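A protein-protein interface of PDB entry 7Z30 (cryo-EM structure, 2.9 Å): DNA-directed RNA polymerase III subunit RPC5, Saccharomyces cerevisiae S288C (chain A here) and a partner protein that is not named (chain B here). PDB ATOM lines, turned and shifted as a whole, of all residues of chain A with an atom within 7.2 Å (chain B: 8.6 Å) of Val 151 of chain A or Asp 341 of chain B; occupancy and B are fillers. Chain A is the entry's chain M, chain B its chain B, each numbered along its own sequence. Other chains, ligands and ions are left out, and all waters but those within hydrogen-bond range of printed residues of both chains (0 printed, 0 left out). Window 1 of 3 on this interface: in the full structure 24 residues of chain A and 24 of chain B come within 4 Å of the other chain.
The side-chain amide nitrogen (NE2) of Gln 178 of chain A sits close to the guanidinium group (NH1) of Arg 343 of chain B (3.3 Å).
The backbone carbonyl oxygen (O) of Ala 339 of chain B is in hydrogen-bond range of the side-chain hydroxyl (OG) of Ser 230 of chain A.
The backbone NH (N) of Val 153 of chain A sits at hydrogen-bond distance from the backbone carbonyl oxygen (O) of Val 176 of chain A, at 2.6 Å.
The backbone carbonyl oxygen of Ile 541 of chain B sits at hydrogen-bond distance from the guanidinium group of Arg 343 of chain B, at 3.2 Å.
OD1 of Asp 540 of chain B sits close to N of Thr 542 of chain B, 3.3 Å away.
Among the printed residues, merely in contact across the chains: Leu 118 of chain A with Leu 340 of chain B (3.5 Å), Val 151 of chain A with Leu 340 of chain B (3.5 Å), Val 151 of chain A with Asp 341 of chain B (3.9 Å), Val 153 of chain A with Asp 341 of chain B (3.99 Å), Val 153 of chain A with Thr 542 of chain B (3.7 Å), Gln 178 of chain A with Thr 542 of chain B (3.6 Å), Ser 230 of chain A with Val 337 of chain B (3.3 Å), Ala 233 of chain A with Ala 339 of chain B (3.99 Å) and His 234 of chain A with Phe 342 of chain B (3.5 Å).
Printed residues of chain A within 4 Å of Asp 341 of chain B: Val 151 (3.9 Å) and Val 153 (3.99 Å).
Gly 150 of chain A touches none of the printed residues of chain B.
No residue of chain B comes within 4 Å of Gly 152 of chain A.
Of the printed residues of chain B, Ala 233 of chain A touches Ala 339 (3.99 Å).
Of the printed residues of chain B, Leu 118 of chain A touches Leu 340 (3.5 Å).
Of the printed residues of chain B, His 234 of chain A touches Phe 342 (3.5 Å).
Of the printed residues of chain B, Ser 230 of chain A touches Val 337 (3.3 Å) and Ala 339 (2.7 Å).
The nearest residue of chain B that does not touch Val 151 of chain A is Phe 342 of chain B (5.8 Å).
Hydrophobic or aromatic side chains of chain B within 4 Å of the printed part of chain A: Val 337, Leu 340 and Phe 342.
Of the 18 printed residues of chain A, 7 touch a printed residue of chain B.
Hydrophobic or aromatic side chains of chain A within 4 Å of the printed part of chain B: Leu 118, Val 151, Val 153, Ala 233 and His 234.
Along chain A the printed residues that touch a printed residue of chain B span positions 118 to 234.
Among the printed residues, 11 pairs touch across the chains.
Among the printed residues, no Asp or Glu carboxylate lies within 4 Å of a Lys or Arg side-chain nitrogen of the other chain.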
ATOM      1  N   SER A 116      14.855  32.433  20.580  1.00  0.00           N
ATOM      2  CA  SER A 116      13.946  31.297  20.486  1.00  0.00           C
ATOM      3  C   SER A 116      14.096  30.298  21.620  1.00  0.00           C
ATOM      4  O   SER A 116      13.149  29.544  21.870  1.00  0.00           O
ATOM      5  CB  SER A 116      14.136  30.564  19.154  1.00  0.00           C
ATOM      6  OG  SER A 116      13.067  29.668  18.912  1.00  0.00           O
ATOM      7  N   HIS A 117      15.234  30.261  22.316  1.00  0.00           N
ATOM      8  CA  HIS A 117      15.463  29.368  23.451  1.00  0.00           C
ATOM      9  C   HIS A 117      15.177  27.913  23.077  1.00  0.00           C
ATOM     10  O   HIS A 117      14.486  27.178  23.785  1.00  0.00           O
ATOM     11  CB  HIS A 117      14.633  29.810  24.659  1.00  0.00           C
ATOM     12  CG  HIS A 117      14.644  31.290  24.885  1.00  0.00           C
ATOM     13  ND1 HIS A 117      15.806  32.031  24.897  1.00  0.00           N
ATOM     14  CD2 HIS A 117      13.636  32.169  25.095  1.00  0.00           C
ATOM     15  CE1 HIS A 117      15.514  33.301  25.113  1.00  0.00           C
ATOM     16  NE2 HIS A 117      14.204  33.412  25.236  1.00  0.00           N
ATOM     17  N   LEU A 118      15.737  27.506  21.943  1.00  0.00           N
ATOM     18  CA  LEU A 118      15.558  26.167  21.398  1.00  0.00           C
ATOM     19  C   LEU A 118      16.841  25.375  21.602  1.00  0.00           C
ATOM     20  O   LEU A 118      17.926  25.839  21.237  1.00  0.00           O
ATOM     21  CB  LEU A 118      15.189  26.231  19.914  1.00  0.00           C
ATOM     22  CG  LEU A 118      14.499  25.042  19.233  1.00  0.00           C
ATOM     23  CD1 LEU A 118      15.383  23.812  19.159  1.00  0.00           C
ATOM     24  CD2 LEU A 118      13.214  24.711  19.959  1.00  0.00           C
ATOM     25  N   TRP A 119      16.712  24.187  22.182  1.00  0.00           N
ATOM     26  CA  TRP A 119      17.849  23.336  22.506  1.00  0.00           C
ATOM     27  C   TRP A 119      17.924  22.174  21.529  1.00  0.00           C
ATOM     28  O   TRP A 119      16.923  21.494  21.286  1.00  0.00           O
ATOM     29  CB  TRP A 119      17.755  22.822  23.939  1.00  0.00           C
ATOM     30  CG  TRP A 119      18.619  23.589  24.857  1.00  0.00           C
ATOM     31  CD1 TRP A 119      18.222  24.414  25.865  1.00  0.00           C
ATOM     32  CD2 TRP A 119      20.046  23.634  24.834  1.00  0.00           C
ATOM     33  NE1 TRP A 119      19.318  24.962  26.483  1.00  0.00           N
ATOM     34  CE2 TRP A 119      20.451  24.499  25.866  1.00  0.00           C
ATOM     35  CE3 TRP A 119      21.022  23.021  24.044  1.00  0.00           C
ATOM     36  CZ2 TRP A 119      21.787  24.766  26.126  1.00  0.00           C
ATOM     37  CZ3 TRP A 119      22.347  23.286  24.305  1.00  0.00           C
ATOM     38  CH2 TRP A 119      22.719  24.150  25.339  1.00  0.00           C
ATOM     39  N   LYS A 149      15.592  17.351  20.889  1.00  0.00           N
ATOM     40  CA  LYS A 149      15.189  18.740  20.741  1.00  0.00           C
ATOM     41  C   LYS A 149      14.147  19.087  21.795  1.00  0.00           C
ATOM     42  O   LYS A 149      13.200  18.325  22.012  1.00  0.00           O
ATOM     43  CB  LYS A 149      14.635  18.996  19.340  1.00  0.00           C
ATOM     44  CG  LYS A 149      14.452  20.457  19.013  1.00  0.00           C
ATOM     45  CD  LYS A 149      13.801  20.644  17.659  1.00  0.00           C
ATOM     46  CE  LYS A 149      12.300  20.820  17.791  1.00  0.00           C
ATOM     47  NZ  LYS A 149      11.702  21.350  16.538  1.00  0.00           N
ATOM     48  N   GLY A 150      14.326  20.235  22.443  1.00  0.00           N
ATOM     49  CA  GLY A 150      13.360  20.699  23.418  1.00  0.00           C
ATOM     50  C   GLY A 150      13.523  22.161  23.777  1.00  0.00           C
ATOM     51  O   GLY A 150      14.620  22.604  24.120  1.00  0.00           O
ATOM     52  N   VAL A 151      12.430  22.915  23.720  1.00  0.00           N
ATOM     53  CA  VAL A 151      12.474  24.349  23.985  1.00  0.00           C
ATOM     54  C   VAL A 151      12.609  24.574  25.485  1.00  0.00           C
ATOM     55  O   VAL A 151      11.924  23.931  26.288  1.00  0.00           O
ATOM     56  CB  VAL A 151      11.231  25.055  23.423  1.00  0.00           C
ATOM     57  CG1 VAL A 151       9.953  24.460  23.999  1.00  0.00           C
ATOM     58  CG2 VAL A 151      11.297  26.552  23.693  1.00  0.00           C
ATOM     59  N   GLY A 152      13.521  25.463  25.868  1.00  0.00           N
ATOM     60  CA  GLY A 152      13.627  25.862  27.255  1.00  0.00           C
ATOM     61  C   GLY A 152      12.417  26.664  27.682  1.00  0.00           C
ATOM     62  O   GLY A 152      12.005  27.591  26.979  1.00  0.00           O
ATOM     63  N   VAL A 153      11.833  26.320  28.826  1.00  0.00           N
ATOM     64  CA  VAL A 153      10.637  26.985  29.329  1.00  0.00           C
ATOM     65  C   VAL A 153      11.026  27.835  30.528  1.00  0.00           C
ATOM     66  O   VAL A 153      11.617  27.335  31.495  1.00  0.00           O
ATOM     67  CB  VAL A 153       9.533  25.971  29.685  1.00  0.00           C
ATOM     68  CG1 VAL A 153       8.912  25.412  28.419  1.00  0.00           C
ATOM     69  CG2 VAL A 153      10.091  24.839  30.531  1.00  0.00           C
ATOM     70  N   GLU A 154      10.712  29.127  30.456  1.00  0.00           N
ATOM     71  CA  GLU A 154      11.074  30.064  31.512  1.00  0.00           C
ATOM     72  C   GLU A 154      10.161  29.866  32.712  1.00  0.00           C
ATOM     73  O   GLU A 154       8.967  30.179  32.655  1.00  0.00           O
ATOM     74  CB  GLU A 154      10.993  31.500  31.003  1.00  0.00           C
ATOM     75  CG  GLU A 154      11.264  32.536  32.081  1.00  0.00           C
ATOM     76  CD  GLU A 154      12.701  32.522  32.563  1.00  0.00           C
ATOM     77  OE1 GLU A 154      13.601  32.230  31.749  1.00  0.00           O
ATOM     78  OE2 GLU A 154      12.929  32.791  33.761  1.00  0.00           O
ATOM     79  N   ARG A 175      15.447  28.738  32.256  1.00  0.00           N
ATOM     80  CA  ARG A 175      14.886  28.054  31.091  1.00  0.00           C
ATOM     81  C   ARG A 175      15.286  26.574  31.050  1.00  0.00           C
ATOM     82  O   ARG A 175      16.035  26.120  30.181  1.00  0.00           O
ATOM     83  CB  ARG A 175      15.300  28.771  29.802  1.00  0.00           C
ATOM     84  CG  ARG A 175      14.626  30.111  29.639  1.00  0.00           C
ATOM     85  CD  ARG A 175      14.233  30.387  28.206  1.00  0.00           C
ATOM     86  NE  ARG A 175      13.272  31.480  28.123  1.00  0.00           N
ATOM     87  CZ  ARG A 175      13.564  32.758  28.327  1.00  0.00           C
ATOM     88  NH1 ARG A 175      14.796  33.150  28.609  1.00  0.00           N
ATOM     89  NH2 ARG A 175      12.596  33.665  28.245  1.00  0.00           N
ATOM     90  N   VAL A 176      14.776  25.833  32.037  1.00  0.00           N
ATOM     91  CA  VAL A 176      14.799  24.376  31.957  1.00  0.00           C
ATOM     92  C   VAL A 176      14.173  23.925  30.642  1.00  0.00           C
ATOM     93  O   VAL A 176      13.257  24.567  30.115  1.00  0.00           O
ATOM     94  CB  VAL A 176      14.082  23.758  33.172  1.00  0.00           C
ATOM     95  CG1 VAL A 176      12.578  23.787  32.984  1.00  0.00           C
ATOM     96  CG2 VAL A 176      14.532  22.329  33.371  1.00  0.00           C
ATOM     97  N   ALA A 177      14.682  22.824  30.094  1.00  0.00           N
ATOM     98  CA  ALA A 177      14.230  22.308  28.807  1.00  0.00           C
ATOM     99  C   ALA A 177      13.977  20.811  28.904  1.00  0.00           C
ATOM    100  O   ALA A 177      14.672  20.104  29.639  1.00  0.00           O
ATOM    101  CB  ALA A 177      15.252  22.597  27.705  1.00  0.00           C
ATOM    102  N   GLN A 178      12.986  20.336  28.153  1.00  0.00           N
ATOM    103  CA  GLN A 178      12.623  18.922  28.079  1.00  0.00           C
ATOM    104  C   GLN A 178      13.020  18.408  26.701  1.00  0.00           C
ATOM    105  O   GLN A 178      12.424  18.792  25.692  1.00  0.00           O
ATOM    106  CB  GLN A 178      11.132  18.732  28.324  1.00  0.00           C
ATOM    107  CG  GLN A 178      10.737  18.670  29.779  1.00  0.00           C
ATOM    108  CD  GLN A 178       9.598  17.705  30.015  1.00  0.00           C
ATOM    109  OE1 GLN A 178       9.563  17.000  31.023  1.00  0.00           O
ATOM    110  NE2 GLN A 178       8.649  17.677  29.088  1.00  0.00           N
ATOM    111  N   LEU A 179      14.002  17.513  26.661  1.00  0.00           N
ATOM    112  CA  LEU A 179      14.602  17.094  25.403  1.00  0.00           C
ATOM    113  C   LEU A 179      14.026  15.758  24.954  1.00  0.00           C
ATOM    114  O   LEU A 179      14.055  14.775  25.702  1.00  0.00           O
ATOM    115  CB  LEU A 179      16.122  17.006  25.547  1.00  0.00           C
ATOM    116  CG  LEU A 179      16.754  18.349  25.917  1.00  0.00           C
ATOM    117  CD1 LEU A 179      17.563  18.227  27.197  1.00  0.00           C
ATOM    118  CD2 LEU A 179      17.594  18.913  24.788  1.00  0.00           C
ATOM    119  N   SER A 230       1.627  32.245  17.665  1.00  0.00           N
ATOM    120  CA  SER A 230       2.410  30.985  17.565  1.00  0.00           C
ATOM    121  C   SER A 230       2.980  30.861  16.150  1.00  0.00           C
ATOM    122  O   SER A 230       4.053  30.247  16.000  1.00  0.00           O
ATOM    123  CB  SER A 230       1.577  29.787  17.932  1.00  0.00           C
ATOM    124  OG  SER A 230       2.384  28.778  18.523  1.00  0.00           O
ATOM    125  N   ALA A 233       6.184  32.534  16.177  1.00  0.00           N
ATOM    126  CA  ALA A 233       7.197  31.806  16.935  1.00  0.00           C
ATOM    127  C   ALA A 233       7.958  30.831  16.041  1.00  0.00           C
ATOM    128  O   ALA A 233       9.195  30.832  16.009  1.00  0.00           O
ATOM    129  CB  ALA A 233       6.547  31.073  18.107  1.00  0.00           C
ATOM    130  N   HIS A 234       7.232  30.007  15.284  1.00  0.00           N
ATOM    131  CA  HIS A 234       7.889  29.065  14.383  1.00  0.00           C
ATOM    132  C   HIS A 234       8.521  29.784  13.196  1.00  0.00           C
ATOM    133  O   HIS A 234       9.558  29.346  12.678  1.00  0.00           O
ATOM    134  CB  HIS A 234       6.892  28.006  13.918  1.00  0.00           C
ATOM    135  CG  HIS A 234       6.388  27.130  15.023  1.00  0.00           C
ATOM    136  ND1 HIS A 234       6.781  25.817  15.171  1.00  0.00           N
ATOM    137  CD2 HIS A 234       5.533  27.384  16.042  1.00  0.00           C
ATOM    138  CE1 HIS A 234       6.183  25.298  16.228  1.00  0.00           C
ATOM    139  NE2 HIS A 234       5.422  26.227  16.775  1.00  0.00           N
ATOM    140  N   ALA B 259       1.731  15.595  17.358  1.00  0.00           N
ATOM    141  CA  ALA B 259       1.789  16.972  16.890  1.00  0.00           C
ATOM    142  C   ALA B 259       2.019  17.959  18.024  1.00  0.00           C
ATOM    143  O   ALA B 259       2.799  18.903  17.856  1.00  0.00           O
ATOM    144  CB  ALA B 259       0.504  17.332  16.146  1.00  0.00           C
ATOM    145  N   CYS B 260       1.371  17.765  19.175  1.00  0.00           N
ATOM    146  CA  CYS B 260       1.517  18.682  20.299  1.00  0.00           C
ATOM    147  C   CYS B 260       2.784  18.425  21.111  1.00  0.00           C
ATOM    148  O   CYS B 260       2.733  18.411  22.347  1.00  0.00           O
ATOM    149  CB  CYS B 260       0.285  18.603  21.203  1.00  0.00           C
ATOM    150  SG  CYS B 260      -1.274  19.001  20.385  1.00  0.00           S
ATOM    151  N   GLY B 261       3.927  18.251  20.449  1.00  0.00           N
ATOM    152  CA  GLY B 261       5.202  18.133  21.120  1.00  0.00           C
ATOM    153  C   GLY B 261       5.478  16.802  21.786  1.00  0.00           C
ATOM    154  O   GLY B 261       6.650  16.480  22.021  1.00  0.00           O
ATOM    155  N   GLN B 298       7.304  15.364  14.844  1.00  0.00           N
ATOM    156  CA  GLN B 298       6.280  16.323  15.235  1.00  0.00           C
ATOM    157  C   GLN B 298       5.707  17.030  14.013  1.00  0.00           C
ATOM    158  O   GLN B 298       4.484  17.124  13.851  1.00  0.00           O
ATOM    159  CB  GLN B 298       6.850  17.328  16.234  1.00  0.00           C
ATOM    160  CG  GLN B 298       6.042  18.600  16.348  1.00  0.00           C
ATOM    161  CD  GLN B 298       6.285  19.337  17.647  1.00  0.00           C
ATOM    162  OE1 GLN B 298       6.973  18.840  18.537  1.00  0.00           O
ATOM    163  NE2 GLN B 298       5.739  20.542  17.752  1.00  0.00           N
ATOM    164  N   THR B 329      -4.397  24.414  15.600  1.00  0.00           N
ATOM    165  CA  THR B 329      -4.186  24.006  16.984  1.00  0.00           C
ATOM    166  C   THR B 329      -4.383  25.177  17.944  1.00  0.00           C
ATOM    167  O   THR B 329      -4.844  24.986  19.075  1.00  0.00           O
ATOM    168  CB  THR B 329      -2.789  23.395  17.132  1.00  0.00           C
ATOM    169  OG1 THR B 329      -2.727  22.168  16.396  1.00  0.00           O
ATOM    170  CG2 THR B 329      -2.457  23.112  18.587  1.00  0.00           C
ATOM    171  N   LEU B 335      -6.917  26.913  25.227  1.00  0.00           N
ATOM    172  CA  LEU B 335      -5.524  26.968  25.669  1.00  0.00           C
ATOM    173  C   LEU B 335      -4.662  27.588  24.570  1.00  0.00           C
ATOM    174  O   LEU B 335      -3.758  26.968  24.008  1.00  0.00           O
ATOM    175  CB  LEU B 335      -5.038  25.578  26.052  1.00  0.00           C
ATOM    176  CG  LEU B 335      -5.585  25.070  27.384  1.00  0.00           C
ATOM    177  CD1 LEU B 335      -5.457  23.562  27.488  1.00  0.00           C
ATOM    178  CD2 LEU B 335      -4.863  25.755  28.527  1.00  0.00           C
ATOM    179  N   THR B 336      -4.969  28.850  24.273  1.00  0.00           N
ATOM    180  CA  THR B 336      -4.275  29.569  23.213  1.00  0.00           C
ATOM    181  C   THR B 336      -2.775  29.586  23.469  1.00  0.00           C
ATOM    182  O   THR B 336      -2.316  30.013  24.532  1.00  0.00           O
ATOM    183  CB  THR B 336      -4.810  30.997  23.110  1.00  0.00           C
ATOM    184  OG1 THR B 336      -4.813  31.603  24.410  1.00  0.00           O
ATOM    185  CG2 THR B 336      -6.225  30.996  22.554  1.00  0.00           C
ATOM    186  N   VAL B 337      -2.014  29.112  22.488  1.00  0.00           N
ATOM    187  CA  VAL B 337      -0.563  29.011  22.585  1.00  0.00           C
ATOM    188  C   VAL B 337       0.040  30.153  21.782  1.00  0.00           C
ATOM    189  O   VAL B 337      -0.291  30.338  20.604  1.00  0.00           O
ATOM    190  CB  VAL B 337      -0.064  27.650  22.076  1.00  0.00           C
ATOM    191  CG1 VAL B 337       1.453  27.636  21.989  1.00  0.00           C
ATOM    192  CG2 VAL B 337      -0.574  26.525  22.967  1.00  0.00           C
ATOM    193  N   GLU B 338       0.919  30.922  22.416  1.00  0.00           N
ATOM    194  CA  GLU B 338       1.566  32.071  21.794  1.00  0.00           C
ATOM    195  C   GLU B 338       3.074  31.866  21.717  1.00  0.00           C
ATOM    196  O   GLU B 338       3.844  32.814  21.555  1.00  0.00           O
ATOM    197  CB  GLU B 338       1.237  33.355  22.550  1.00  0.00           C
ATOM    198  CG  GLU B 338      -0.204  33.809  22.407  1.00  0.00           C
ATOM    199  CD  GLU B 338      -0.462  34.523  21.096  1.00  0.00           C
ATOM    200  OE1 GLU B 338       0.447  35.236  20.618  1.00  0.00           O
ATOM    201  OE2 GLU B 338      -1.573  34.375  20.546  1.00  0.00           O
ATOM    202  N   ALA B 339       3.508  30.616  21.818  1.00  0.00           N
ATOM    203  CA  ALA B 339       4.925  30.284  21.840  1.00  0.00           C
ATOM    204  C   ALA B 339       5.106  28.936  21.153  1.00  0.00           C
ATOM    205  O   ALA B 339       4.213  28.457  20.446  1.00  0.00           O
ATOM    206  CB  ALA B 339       5.465  30.287  23.274  1.00  0.00           C
ATOM    207  N   LEU B 340       6.268  28.323  21.355  1.00  0.00           N
ATOM    208  CA  LEU B 340       6.621  27.087  20.674  1.00  0.00           C
ATOM    209  C   LEU B 340       6.566  25.872  21.604  1.00  0.00           C
ATOM    210  O   LEU B 340       6.913  24.762  21.186  1.00  0.00           O
ATOM    211  CB  LEU B 340       8.005  27.252  20.028  1.00  0.00           C
ATOM    212  CG  LEU B 340       8.777  26.149  19.299  1.00  0.00           C
ATOM    213  CD1 LEU B 340       9.449  26.710  18.059  1.00  0.00           C
ATOM    214  CD2 LEU B 340       9.805  25.545  20.219  1.00  0.00           C
ATOM    215  N   ASP B 341       6.090  26.046  22.835  1.00  0.00           N
ATOM    216  CA  ASP B 341       5.936  24.952  23.788  1.00  0.00           C
ATOM    217  C   ASP B 341       4.480  24.495  23.793  1.00  0.00           C
ATOM    218  O   ASP B 341       3.571  25.302  24.011  1.00  0.00           O
ATOM    219  CB  ASP B 341       6.377  25.383  25.187  1.00  0.00           C
ATOM    220  CG  ASP B 341       5.639  26.613  25.681  1.00  0.00           C
ATOM    221  OD1 ASP B 341       5.231  27.442  24.838  1.00  0.00           O
ATOM    222  OD2 ASP B 341       5.467  26.751  26.909  1.00  0.00           O
ATOM    223  N   PHE B 342       4.262  23.202  23.533  1.00  0.00           N
ATOM    224  CA  PHE B 342       2.925  22.635  23.392  1.00  0.00           C
ATOM    225  C   PHE B 342       2.556  21.720  24.557  1.00  0.00           C
ATOM    226  O   PHE B 342       1.599  20.944  24.452  1.00  0.00           O
ATOM    227  CB  PHE B 342       2.790  21.871  22.070  1.00  0.00           C
ATOM    228  CG  PHE B 342       2.883  22.729  20.823  1.00  0.00           C
ATOM    229  CD1 PHE B 342       3.705  23.843  20.758  1.00  0.00           C
ATOM    230  CD2 PHE B 342       2.146  22.394  19.699  1.00  0.00           C
ATOM    231  CE1 PHE B 342       3.780  24.609  19.613  1.00  0.00           C
ATOM    232  CE2 PHE B 342       2.218  23.156  18.548  1.00  0.00           C
ATOM    233  CZ  PHE B 342       3.036  24.264  18.506  1.00  0.00           C
ATOM    234  N   ARG B 343       3.293  21.805  25.668  1.00  0.00           N
ATOM    235  CA  ARG B 343       3.101  20.875  26.775  1.00  0.00           C
ATOM    236  C   ARG B 343       1.708  20.982  27.386  1.00  0.00           C
ATOM    237  O   ARG B 343       1.105  19.959  27.729  1.00  0.00           O
ATOM    238  CB  ARG B 343       4.165  21.118  27.844  1.00  0.00           C
ATOM    239  CG  ARG B 343       4.090  20.175  29.032  1.00  0.00           C
ATOM    240  CD  ARG B 343       4.805  18.865  28.757  1.00  0.00           C
ATOM    241  NE  ARG B 343       5.012  18.101  29.980  1.00  0.00           N
ATOM    242  CZ  ARG B 343       5.453  16.850  30.020  1.00  0.00           C
ATOM    243  NH1 ARG B 343       5.762  16.192  28.916  1.00  0.00           N
ATOM    244  NH2 ARG B 343       5.586  16.246  31.196  1.00  0.00           N
ATOM    245  N   GLU B 344       1.186  22.201  27.538  1.00  0.00           N
ATOM    246  CA  GLU B 344      -0.109  22.384  28.189  1.00  0.00           C
ATOM    247  C   GLU B 344      -1.228  21.723  27.392  1.00  0.00           C
ATOM    248  O   GLU B 344      -2.008  20.927  27.935  1.00  0.00           O
ATOM    249  CB  GLU B 344      -0.388  23.875  28.376  1.00  0.00           C
ATOM    250  CG  GLU B 344      -1.335  24.207  29.516  1.00  0.00           C
ATOM    251  CD  GLU B 344      -0.933  25.472  30.255  1.00  0.00           C
ATOM    252  OE1 GLU B 344       0.253  25.596  30.627  1.00  0.00           O
ATOM    253  OE2 GLU B 344      -1.803  26.346  30.461  1.00  0.00           O
ATOM    254  N   LYS B 345      -1.321  22.040  26.097  1.00  0.00           N
ATOM    255  CA  LYS B 345      -2.342  21.427  25.254  1.00  0.00           C
ATOM    256  C   LYS B 345      -2.129  19.925  25.144  1.00  0.00           C
ATOM    257  O   LYS B 345      -3.095  19.153  25.090  1.00  0.00           O
ATOM    258  CB  LYS B 345      -2.334  22.067  23.867  1.00  0.00           C
ATOM    259  CG  LYS B 345      -3.610  21.841  23.072  1.00  0.00           C
ATOM    260  CD  LYS B 345      -3.745  22.850  21.946  1.00  0.00           C
ATOM    261  CE  LYS B 345      -4.046  24.242  22.463  1.00  0.00           C
ATOM    262  NZ  LYS B 345      -5.499  24.554  22.431  1.00  0.00           N
ATOM    263  N   ALA B 346      -0.868  19.490  25.102  1.00  0.00           N
ATOM    264  CA  ALA B 346      -0.581  18.063  25.015  1.00  0.00           C
ATOM    265  C   ALA B 346      -1.116  17.320  26.232  1.00  0.00           C
ATOM    266  O   ALA B 346      -1.760  16.274  26.100  1.00  0.00           O
ATOM    267  CB  ALA B 346       0.923  17.845  24.868  1.00  0.00           C
ATOM    268  N   ASP B 540       5.236  22.797  38.109  1.00  0.00           N
ATOM    269  CA  ASP B 540       4.661  23.003  36.788  1.00  0.00           C
ATOM    270  C   ASP B 540       4.793  21.739  35.943  1.00  0.00           C
ATOM    271  O   ASP B 540       5.705  20.929  36.131  1.00  0.00           O
ATOM    272  CB  ASP B 540       5.350  24.181  36.096  1.00  0.00           C
ATOM    273  CG  ASP B 540       4.588  24.683  34.881  1.00  0.00           C
ATOM    274  OD1 ASP B 540       3.845  23.899  34.257  1.00  0.00           O
ATOM    275  OD2 ASP B 540       4.740  25.877  34.549  1.00  0.00           O
ATOM    276  N   ILE B 541       3.852  21.568  35.012  1.00  0.00           N
ATOM    277  CA  ILE B 541       3.864  20.400  34.143  1.00  0.00           C
ATOM    278  C   ILE B 541       5.102  20.367  33.259  1.00  0.00           C
ATOM    279  O   ILE B 541       5.608  19.284  32.947  1.00  0.00           O
ATOM    280  CB  ILE B 541       2.573  20.347  33.300  1.00  0.00           C
ATOM    281  CG1 ILE B 541       2.427  21.608  32.450  1.00  0.00           C
ATOM    282  CG2 ILE B 541       1.362  20.149  34.191  1.00  0.00           C
ATOM    283  CD1 ILE B 541       1.398  21.481  31.359  1.00  0.00           C
ATOM    284  N   THR B 542       5.608  21.529  32.844  1.00  0.00           N
ATOM    285  CA  THR B 542       6.844  21.579  32.075  1.00  0.00           C
ATOM    286  C   THR B 542       8.047  21.088  32.868  1.00  0.00           C
ATOM    287  O   THR B 542       9.038  20.666  32.264  1.00  0.00           O
ATOM    288  CB  THR B 542       7.100  23.004  31.582  1.00  0.00           C
ATOM    289  OG1 THR B 542       6.659  23.941  32.572  1.00  0.00           O
ATOM    290  CG2 THR B 542       6.353  23.257  30.284  1.00  0.00           C
